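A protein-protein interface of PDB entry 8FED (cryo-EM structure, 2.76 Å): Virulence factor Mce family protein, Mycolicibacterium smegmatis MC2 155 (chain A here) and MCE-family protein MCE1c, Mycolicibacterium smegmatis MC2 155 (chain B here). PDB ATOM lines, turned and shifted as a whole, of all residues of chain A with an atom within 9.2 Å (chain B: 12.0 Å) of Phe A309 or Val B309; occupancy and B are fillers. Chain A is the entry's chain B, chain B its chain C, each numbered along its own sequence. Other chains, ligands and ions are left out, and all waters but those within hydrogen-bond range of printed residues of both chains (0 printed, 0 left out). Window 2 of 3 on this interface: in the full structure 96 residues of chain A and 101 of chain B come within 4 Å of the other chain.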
ATOM      1  N   ALA A 299       9.961 -24.085  -7.188  1.00  0.00           N
ATOM      2  CA  ALA A 299       9.039 -22.981  -7.423  1.00  0.00           C
ATOM      3  C   ALA A 299       9.715 -21.841  -8.173  1.00  0.00           C
ATOM      4  O   ALA A 299       9.361 -21.555  -9.320  1.00  0.00           O
ATOM      5  CB  ALA A 299       8.467 -22.470  -6.101  1.00  0.00           C
ATOM      6  N   GLY A 300      10.696 -21.187  -7.544  1.00  0.00           N
ATOM      7  CA  GLY A 300      11.360 -20.054  -8.147  1.00  0.00           C
ATOM      8  C   GLY A 300      12.868 -20.151  -7.986  1.00  0.00           C
ATOM      9  O   GLY A 300      13.379 -20.939  -7.189  1.00  0.00           O
ATOM     10  N   GLY A 301      13.570 -19.335  -8.768  1.00  0.00           N
ATOM     11  CA  GLY A 301      15.017 -19.344  -8.765  1.00  0.00           C
ATOM     12  C   GLY A 301      15.663 -20.362  -9.679  1.00  0.00           C
ATOM     13  O   GLY A 301      16.894 -20.489  -9.661  1.00  0.00           O
ATOM     14  N   TYR A 303      14.461 -20.654 -13.150  1.00  0.00           N
ATOM     15  CA  TYR A 303      14.398 -20.075 -14.485  1.00  0.00           C
ATOM     16  C   TYR A 303      15.298 -18.860 -14.653  1.00  0.00           C
ATOM     17  O   TYR A 303      15.445 -18.372 -15.777  1.00  0.00           O
ATOM     18  CB  TYR A 303      12.958 -19.686 -14.828  1.00  0.00           C
ATOM     19  CG  TYR A 303      12.016 -20.856 -15.005  1.00  0.00           C
ATOM     20  CD1 TYR A 303      12.496 -22.148 -15.162  1.00  0.00           C
ATOM     21  CD2 TYR A 303      10.643 -20.663 -15.030  1.00  0.00           C
ATOM     22  CE1 TYR A 303      11.633 -23.213 -15.328  1.00  0.00           C
ATOM     23  CE2 TYR A 303       9.775 -21.719 -15.198  1.00  0.00           C
ATOM     24  CZ  TYR A 303      10.274 -22.992 -15.345  1.00  0.00           C
ATOM     25  OH  TYR A 303       9.407 -24.046 -15.512  1.00  0.00           O
ATOM     26  N   PHE A 306      14.851 -14.689 -10.701  1.00  0.00           N
ATOM     27  CA  PHE A 306      13.542 -14.221 -10.271  1.00  0.00           C
ATOM     28  C   PHE A 306      12.714 -15.363  -9.705  1.00  0.00           C
ATOM     29  O   PHE A 306      12.913 -16.529 -10.053  1.00  0.00           O
ATOM     30  CB  PHE A 306      12.796 -13.555 -11.435  1.00  0.00           C
ATOM     31  CG  PHE A 306      12.824 -14.352 -12.710  1.00  0.00           C
ATOM     32  CD1 PHE A 306      11.943 -15.400 -12.914  1.00  0.00           C
ATOM     33  CD2 PHE A 306      13.725 -14.041 -13.711  1.00  0.00           C
ATOM     34  CE1 PHE A 306      11.967 -16.129 -14.085  1.00  0.00           C
ATOM     35  CE2 PHE A 306      13.753 -14.766 -14.886  1.00  0.00           C
ATOM     36  CZ  PHE A 306      12.872 -15.812 -15.072  1.00  0.00           C
ATOM     37  N   PHE A 307      11.781 -15.010  -8.821  1.00  0.00           N
ATOM     38  CA  PHE A 307      10.753 -15.934  -8.369  1.00  0.00           C
ATOM     39  C   PHE A 307       9.682 -16.089  -9.443  1.00  0.00           C
ATOM     40  O   PHE A 307       9.491 -15.219 -10.294  1.00  0.00           O
ATOM     41  CB  PHE A 307      10.103 -15.441  -7.076  1.00  0.00           C
ATOM     42  CG  PHE A 307      10.959 -15.605  -5.857  1.00  0.00           C
ATOM     43  CD1 PHE A 307      11.912 -14.657  -5.532  1.00  0.00           C
ATOM     44  CD2 PHE A 307      10.793 -16.693  -5.021  1.00  0.00           C
ATOM     45  CE1 PHE A 307      12.695 -14.800  -4.404  1.00  0.00           C
ATOM     46  CE2 PHE A 307      11.573 -16.841  -3.892  1.00  0.00           C
ATOM     47  CZ  PHE A 307      12.525 -15.894  -3.583  1.00  0.00           C
ATOM     48  N   ASN A 308       8.970 -17.207  -9.390  1.00  0.00           N
ATOM     49  CA  ASN A 308       7.872 -17.473 -10.312  1.00  0.00           C
ATOM     50  C   ASN A 308       6.544 -17.270  -9.594  1.00  0.00           C
ATOM     51  O   ASN A 308       6.225 -18.009  -8.658  1.00  0.00           O
ATOM     52  CB  ASN A 308       7.960 -18.889 -10.876  1.00  0.00           C
ATOM     53  CG  ASN A 308       9.049 -19.036 -11.910  1.00  0.00           C
ATOM     54  OD1 ASN A 308      10.217 -19.231 -11.577  1.00  0.00           O
ATOM     55  ND2 ASN A 308       8.672 -18.944 -13.176  1.00  0.00           N
ATOM     56  N   PHE A 309       5.775 -16.280 -10.034  1.00  0.00           N
ATOM     57  CA  PHE A 309       4.435 -16.030  -9.522  1.00  0.00           C
ATOM     58  C   PHE A 309       3.418 -16.259 -10.630  1.00  0.00           C
ATOM     59  O   PHE A 309       3.679 -15.953 -11.795  1.00  0.00           O
ATOM     60  CB  PHE A 309       4.286 -14.605  -8.979  1.00  0.00           C
ATOM     61  CG  PHE A 309       4.864 -14.405  -7.604  1.00  0.00           C
ATOM     62  CD1 PHE A 309       5.612 -15.392  -6.992  1.00  0.00           C
ATOM     63  CD2 PHE A 309       4.639 -13.225  -6.918  1.00  0.00           C
ATOM     64  CE1 PHE A 309       6.136 -15.203  -5.730  1.00  0.00           C
ATOM     65  CE2 PHE A 309       5.159 -13.032  -5.655  1.00  0.00           C
ATOM     66  CZ  PHE A 309       5.908 -14.021  -5.061  1.00  0.00           C
ATOM     67  N   TYR A 310       2.258 -16.800 -10.263  1.00  0.00           N
ATOM     68  CA  TYR A 310       1.168 -17.055 -11.203  1.00  0.00           C
ATOM     69  C   TYR A 310      -0.110 -16.473 -10.609  1.00  0.00           C
ATOM     70  O   TYR A 310      -0.784 -17.129  -9.810  1.00  0.00           O
ATOM     71  CB  TYR A 310       1.017 -18.542 -11.490  1.00  0.00           C
ATOM     72  CG  TYR A 310       0.085 -18.862 -12.637  1.00  0.00           C
ATOM     73  CD1 TYR A 310      -1.292 -18.871 -12.465  1.00  0.00           C
ATOM     74  CD2 TYR A 310       0.585 -19.159 -13.895  1.00  0.00           C
ATOM     75  CE1 TYR A 310      -2.140 -19.164 -13.513  1.00  0.00           C
ATOM     76  CE2 TYR A 310      -0.259 -19.453 -14.948  1.00  0.00           C
ATOM     77  CZ  TYR A 310      -1.619 -19.456 -14.750  1.00  0.00           C
ATOM     78  OH  TYR A 310      -2.463 -19.749 -15.795  1.00  0.00           O
ATOM     79  N   ALA A 311      -0.447 -15.248 -11.002  1.00  0.00           N
ATOM     80  CA  ALA A 311      -1.607 -14.549 -10.457  1.00  0.00           C
ATOM     81  C   ALA A 311      -2.859 -15.064 -11.154  1.00  0.00           C
ATOM     82  O   ALA A 311      -3.168 -14.664 -12.277  1.00  0.00           O
ATOM     83  CB  ALA A 311      -1.455 -13.043 -10.631  1.00  0.00           C
ATOM     84  N   CYS A 312      -3.592 -15.958 -10.485  1.00  0.00           N
ATOM     85  CA  CYS A 312      -4.806 -16.506 -11.082  1.00  0.00           C
ATOM     86  C   CYS A 312      -5.959 -15.516 -11.057  1.00  0.00           C
ATOM     87  O   CYS A 312      -6.780 -15.507 -11.981  1.00  0.00           O
ATOM     88  CB  CYS A 312      -5.229 -17.791 -10.366  1.00  0.00           C
ATOM     89  SG  CYS A 312      -4.644 -19.305 -11.145  1.00  0.00           S
ATOM     90  N   LEU A 314      -6.715 -11.394 -10.223  1.00  0.00           N
ATOM     91  CA  LEU A 314      -6.279 -10.056  -9.858  1.00  0.00           C
ATOM     92  C   LEU A 314      -7.488  -9.134  -9.881  1.00  0.00           C
ATOM     93  O   LEU A 314      -8.310  -9.191 -10.812  1.00  0.00           O
ATOM     94  CB  LEU A 314      -5.165  -9.533 -10.779  1.00  0.00           C
ATOM     95  CG  LEU A 314      -5.364  -9.343 -12.283  1.00  0.00           C
ATOM     96  CD1 LEU A 314      -5.780  -7.917 -12.612  1.00  0.00           C
ATOM     97  CD2 LEU A 314      -4.100  -9.722 -13.039  1.00  0.00           C
ATOM     98  N   ARG A 339      -4.815 -24.884 -12.849  1.00  0.00           N
ATOM     99  CA  ARG A 339      -3.838 -25.118 -11.795  1.00  0.00           C
ATOM    100  C   ARG A 339      -4.289 -24.565 -10.451  1.00  0.00           C
ATOM    101  O   ARG A 339      -3.786 -25.011  -9.415  1.00  0.00           O
ATOM    102  CB  ARG A 339      -2.490 -24.509 -12.178  1.00  0.00           C
ATOM    103  CG  ARG A 339      -2.548 -23.023 -12.442  1.00  0.00           C
ATOM    104  CD  ARG A 339      -1.166 -22.419 -12.590  1.00  0.00           C
ATOM    105  NE  ARG A 339      -0.427 -22.387 -11.333  1.00  0.00           N
ATOM    106  CZ  ARG A 339       0.535 -23.236 -11.007  1.00  0.00           C
ATOM    107  NH1 ARG A 339       0.903 -24.210 -11.821  1.00  0.00           N
ATOM    108  NH2 ARG A 339       1.154 -23.097  -9.838  1.00  0.00           N
ATOM    109  N   LEU B 294      17.698 -19.967  -4.440  1.00  0.00           N
ATOM    110  CA  LEU B 294      16.593 -19.138  -3.969  1.00  0.00           C
ATOM    111  C   LEU B 294      17.080 -17.774  -3.501  1.00  0.00           C
ATOM    112  O   LEU B 294      16.448 -16.752  -3.787  1.00  0.00           O
ATOM    113  CB  LEU B 294      15.844 -19.847  -2.841  1.00  0.00           C
ATOM    114  CG  LEU B 294      14.318 -19.771  -2.881  1.00  0.00           C
ATOM    115  CD1 LEU B 294      13.769 -20.562  -4.050  1.00  0.00           C
ATOM    116  CD2 LEU B 294      13.715 -20.249  -1.575  1.00  0.00           C
ATOM    117  N   ALA B 297      17.769 -14.661  -6.243  1.00  0.00           N
ATOM    118  CA  ALA B 297      16.814 -13.704  -6.800  1.00  0.00           C
ATOM    119  C   ALA B 297      16.812 -12.399  -6.021  1.00  0.00           C
ATOM    120  O   ALA B 297      16.803 -11.310  -6.605  1.00  0.00           O
ATOM    121  CB  ALA B 297      15.413 -14.313  -6.825  1.00  0.00           C
ATOM    122  N   LEU B 298      16.826 -12.493  -4.698  1.00  0.00           N
ATOM    123  CA  LEU B 298      16.838 -11.338  -3.805  1.00  0.00           C
ATOM    124  C   LEU B 298      18.264 -10.915  -3.430  1.00  0.00           C
ATOM    125  O   LEU B 298      18.656 -10.816  -2.272  1.00  0.00           O
ATOM    126  CB  LEU B 298      15.930 -11.650  -2.617  1.00  0.00           C
ATOM    127  CG  LEU B 298      16.103 -12.806  -1.614  1.00  0.00           C
ATOM    128  CD1 LEU B 298      17.092 -12.656  -0.486  1.00  0.00           C
ATOM    129  CD2 LEU B 298      14.731 -13.181  -1.082  1.00  0.00           C
ATOM    130  N   TYR B 303      15.036  -5.620  -2.694  1.00  0.00           N
ATOM    131  CA  TYR B 303      13.776  -6.131  -3.224  1.00  0.00           C
ATOM    132  C   TYR B 303      14.025  -7.569  -3.667  1.00  0.00           C
ATOM    133  O   TYR B 303      15.106  -8.124  -3.438  1.00  0.00           O
ATOM    134  CB  TYR B 303      13.251  -5.257  -4.365  1.00  0.00           C
ATOM    135  CG  TYR B 303      14.336  -4.591  -5.184  1.00  0.00           C
ATOM    136  CD1 TYR B 303      15.077  -5.308  -6.113  1.00  0.00           C
ATOM    137  CD2 TYR B 303      14.615  -3.241  -5.028  1.00  0.00           C
ATOM    138  CE1 TYR B 303      16.066  -4.698  -6.861  1.00  0.00           C
ATOM    139  CE2 TYR B 303      15.602  -2.626  -5.768  1.00  0.00           C
ATOM    140  CZ  TYR B 303      16.323  -3.357  -6.681  1.00  0.00           C
ATOM    141  OH  TYR B 303      17.303  -2.738  -7.416  1.00  0.00           O
ATOM    142  N   PHE B 304      13.027  -8.179  -4.298  1.00  0.00           N
ATOM    143  CA  PHE B 304      13.188  -9.498  -4.896  1.00  0.00           C
ATOM    144  C   PHE B 304      12.413  -9.551  -6.201  1.00  0.00           C
ATOM    145  O   PHE B 304      11.266  -9.103  -6.264  1.00  0.00           O
ATOM    146  CB  PHE B 304      12.725 -10.607  -3.938  1.00  0.00           C
ATOM    147  CG  PHE B 304      11.258 -10.573  -3.617  1.00  0.00           C
ATOM    148  CD1 PHE B 304      10.769  -9.722  -2.644  1.00  0.00           C
ATOM    149  CD2 PHE B 304      10.371 -11.411  -4.270  1.00  0.00           C
ATOM    150  CE1 PHE B 304       9.425  -9.692  -2.346  1.00  0.00           C
ATOM    151  CE2 PHE B 304       9.026 -11.387  -3.970  1.00  0.00           C
ATOM    152  CZ  PHE B 304       8.554 -10.526  -3.011  1.00  0.00           C
ATOM    153  N   LYS B 305      13.038 -10.089  -7.241  1.00  0.00           N
ATOM    154  CA  LYS B 305      12.398 -10.133  -8.544  1.00  0.00           C
ATOM    155  C   LYS B 305      11.297 -11.184  -8.572  1.00  0.00           C
ATOM    156  O   LYS B 305      11.351 -12.193  -7.865  1.00  0.00           O
ATOM    157  CB  LYS B 305      13.427 -10.414  -9.631  1.00  0.00           C
ATOM    158  CG  LYS B 305      14.611  -9.469  -9.600  1.00  0.00           C
ATOM    159  CD  LYS B 305      15.566  -9.740 -10.741  1.00  0.00           C
ATOM    160  CE  LYS B 305      16.905  -9.091 -10.477  1.00  0.00           C
ATOM    161  NZ  LYS B 305      16.723  -7.688 -10.030  1.00  0.00           N
ATOM    162  N   VAL B 306      10.285 -10.934  -9.401  1.00  0.00           N
ATOM    163  CA  VAL B 306       9.160 -11.846  -9.583  1.00  0.00           C
ATOM    164  C   VAL B 306       8.788 -11.874 -11.057  1.00  0.00           C
ATOM    165  O   VAL B 306       8.869 -10.855 -11.748  1.00  0.00           O
ATOM    166  CB  VAL B 306       7.941 -11.442  -8.728  1.00  0.00           C
ATOM    167  CG1 VAL B 306       8.163 -11.800  -7.279  1.00  0.00           C
ATOM    168  CG2 VAL B 306       7.664  -9.958  -8.866  1.00  0.00           C
ATOM    169  N   MET B 307       8.387 -13.043 -11.540  1.00  0.00           N
ATOM    170  CA  MET B 307       7.945 -13.214 -12.921  1.00  0.00           C
ATOM    171  C   MET B 307       6.428 -13.387 -12.905  1.00  0.00           C
ATOM    172  O   MET B 307       5.914 -14.504 -12.821  1.00  0.00           O
ATOM    173  CB  MET B 307       8.633 -14.404 -13.581  1.00  0.00           C
ATOM    174  CG  MET B 307       8.207 -14.643 -15.022  1.00  0.00           C
ATOM    175  SD  MET B 307       8.833 -16.190 -15.702  1.00  0.00           S
ATOM    176  CE  MET B 307       8.105 -16.158 -17.336  1.00  0.00           C
ATOM    177  N   LEU B 308       5.712 -12.272 -12.983  1.00  0.00           N
ATOM    178  CA  LEU B 308       4.252 -12.298 -13.023  1.00  0.00           C
ATOM    179  C   LEU B 308       3.826 -12.782 -14.402  1.00  0.00           C
ATOM    180  O   LEU B 308       3.803 -12.009 -15.362  1.00  0.00           O
ATOM    181  CB  LEU B 308       3.685 -10.917 -12.723  1.00  0.00           C
ATOM    182  CG  LEU B 308       4.385 -10.094 -11.639  1.00  0.00           C
ATOM    183  CD1 LEU B 308       3.795  -8.697 -11.570  1.00  0.00           C
ATOM    184  CD2 LEU B 308       4.286 -10.776 -10.289  1.00  0.00           C
ATOM    185  N   VAL B 309       3.506 -14.073 -14.509  1.00  0.00           N
ATOM    186  CA  VAL B 309       3.121 -14.641 -15.800  1.00  0.00           C
ATOM    187  C   VAL B 309       1.838 -13.998 -16.309  1.00  0.00           C
ATOM    188  O   VAL B 309       1.735 -13.628 -17.486  1.00  0.00           O
ATOM    189  CB  VAL B 309       2.988 -16.172 -15.693  1.00  0.00           C
ATOM    190  CG1 VAL B 309       2.434 -16.754 -16.983  1.00  0.00           C
ATOM    191  CG2 VAL B 309       4.335 -16.796 -15.363  1.00  0.00           C
ATOM    192  N   ASN B 310       0.849 -13.840 -15.437  1.00  0.00           N
ATOM    193  CA  ASN B 310      -0.413 -13.223 -15.825  1.00  0.00           C
ATOM    194  C   ASN B 310      -0.366 -11.707 -15.660  1.00  0.00           C
ATOM    195  O   ASN B 310      -1.367 -11.019 -15.862  1.00  0.00           O
ATOM    196  CB  ASN B 310      -1.565 -13.807 -15.008  1.00  0.00           C
ATOM    197  CG  ASN B 310      -1.734 -15.294 -15.225  1.00  0.00           C
ATOM    198  OD1 ASN B 310      -1.381 -15.823 -16.279  1.00  0.00           O
ATOM    199  ND2 ASN B 310      -2.275 -15.979 -14.228  1.00  0.00           N
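Of the 13 printed residues of chain A, 8 touch a printed residue of chain B. Among the printed residues, 17 pairs touch across the chains. Among the printed residues, no Asp or Glu carboxylate lies within 4 Å of a Lys or Arg side-chain nitrogen of the other chain.
The backbone NH (N) of Phe A307 is in hydrogen-bond range of the backbone carbonyl oxygen (O) of Lys B305, at 3.0 Å. N of Met B307 sits at hydrogen-bond distance from O of Phe A307. The side-chain amide nitrogen (ND2) of Asn A308 sits at hydrogen-bond distance from the side-chain sulfur (SD) of Met B307 (3.7 Å). The backbone carbonyl oxygen (O) of Met B307 lies within hydrogen-bond range of the backbone NH (N) of Phe A309 (3.3 Å). N of Val B309 is in hydrogen-bond range of O of Phe A309 (3.3 Å). O of Ala A311 sits at hydrogen-bond distance from ND2 of Asn B310 (2.5 Å).
CD1 of Leu B294 touches O of Gly A300 (3.2 Å). Ala B297 touches Phe A306 (CB to CA, 3.9 Å). Lys B305 touches Phe A306 (CB to CB, 3.7 Å). CD1 of Phe A306 touches CB of Met B307, 3.5 Å away. Phe A307 touches Ala B297 (CE1 to CB, 3.7 Å). Phe A307 touches Phe B304. CE2 of Phe A309 touches CG1 of Val B306 (3.6 Å). CA of Leu B308 touches O of Phe A309, at 3.9 Å. Tyr A310 touches Asn B310 (CE1 to ND2, 3.3 Å). N of Cys A312 touches ND2 of Asn B310 (3.97 Å).
Phe A309 touches just these residues of chain B: Val B306, Met B307, Leu B308 and Val B309. Val B309 touches one residue of chain A. Ala A311 touches just one residue of chain B: Asn B310 (2.5 Å). Met B307 touches just these residues of chain A: Phe A306, Phe A307, Asn A308 and Phe A309. Asn B310 touches just these residues of chain A: Tyr A310, Ala A311 and Cys A312. Of the printed residues of chain A, Leu B294 touches Gly A300 (3.2 Å). Printed residues of chain A within 4 Å of Lys B305: Phe A306 (3.7 Å) and Phe A307 (3.0 Å). Of the printed residues of chain B, Gly A300 touches Leu B294. Of the printed residues of chain B, Phe A306 touches Ala B297 (3.9 Å), Lys B305 (3.7 Å) and Met B307 (3.5 Å). The nearest residue of chain B that does not touch Phe A309 is Phe B304 (4.2 Å). The nearest residue of chain A that does not touch Val B309 is Tyr A310 (4.2 Å). The nearest printed residue of chain A that does not touch Leu B308 is Phe A307 (5.5 Å).
The side-chain amide oxygen (OD1) of Asn A308 lies close to the backbone carbonyl oxygen (O) of Ala A299, at 3.4 Å. The backbone NH of Gly A301 lies within hydrogen-bond range of the backbone carbonyl oxygen of Phe A306, at 3.2 Å.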
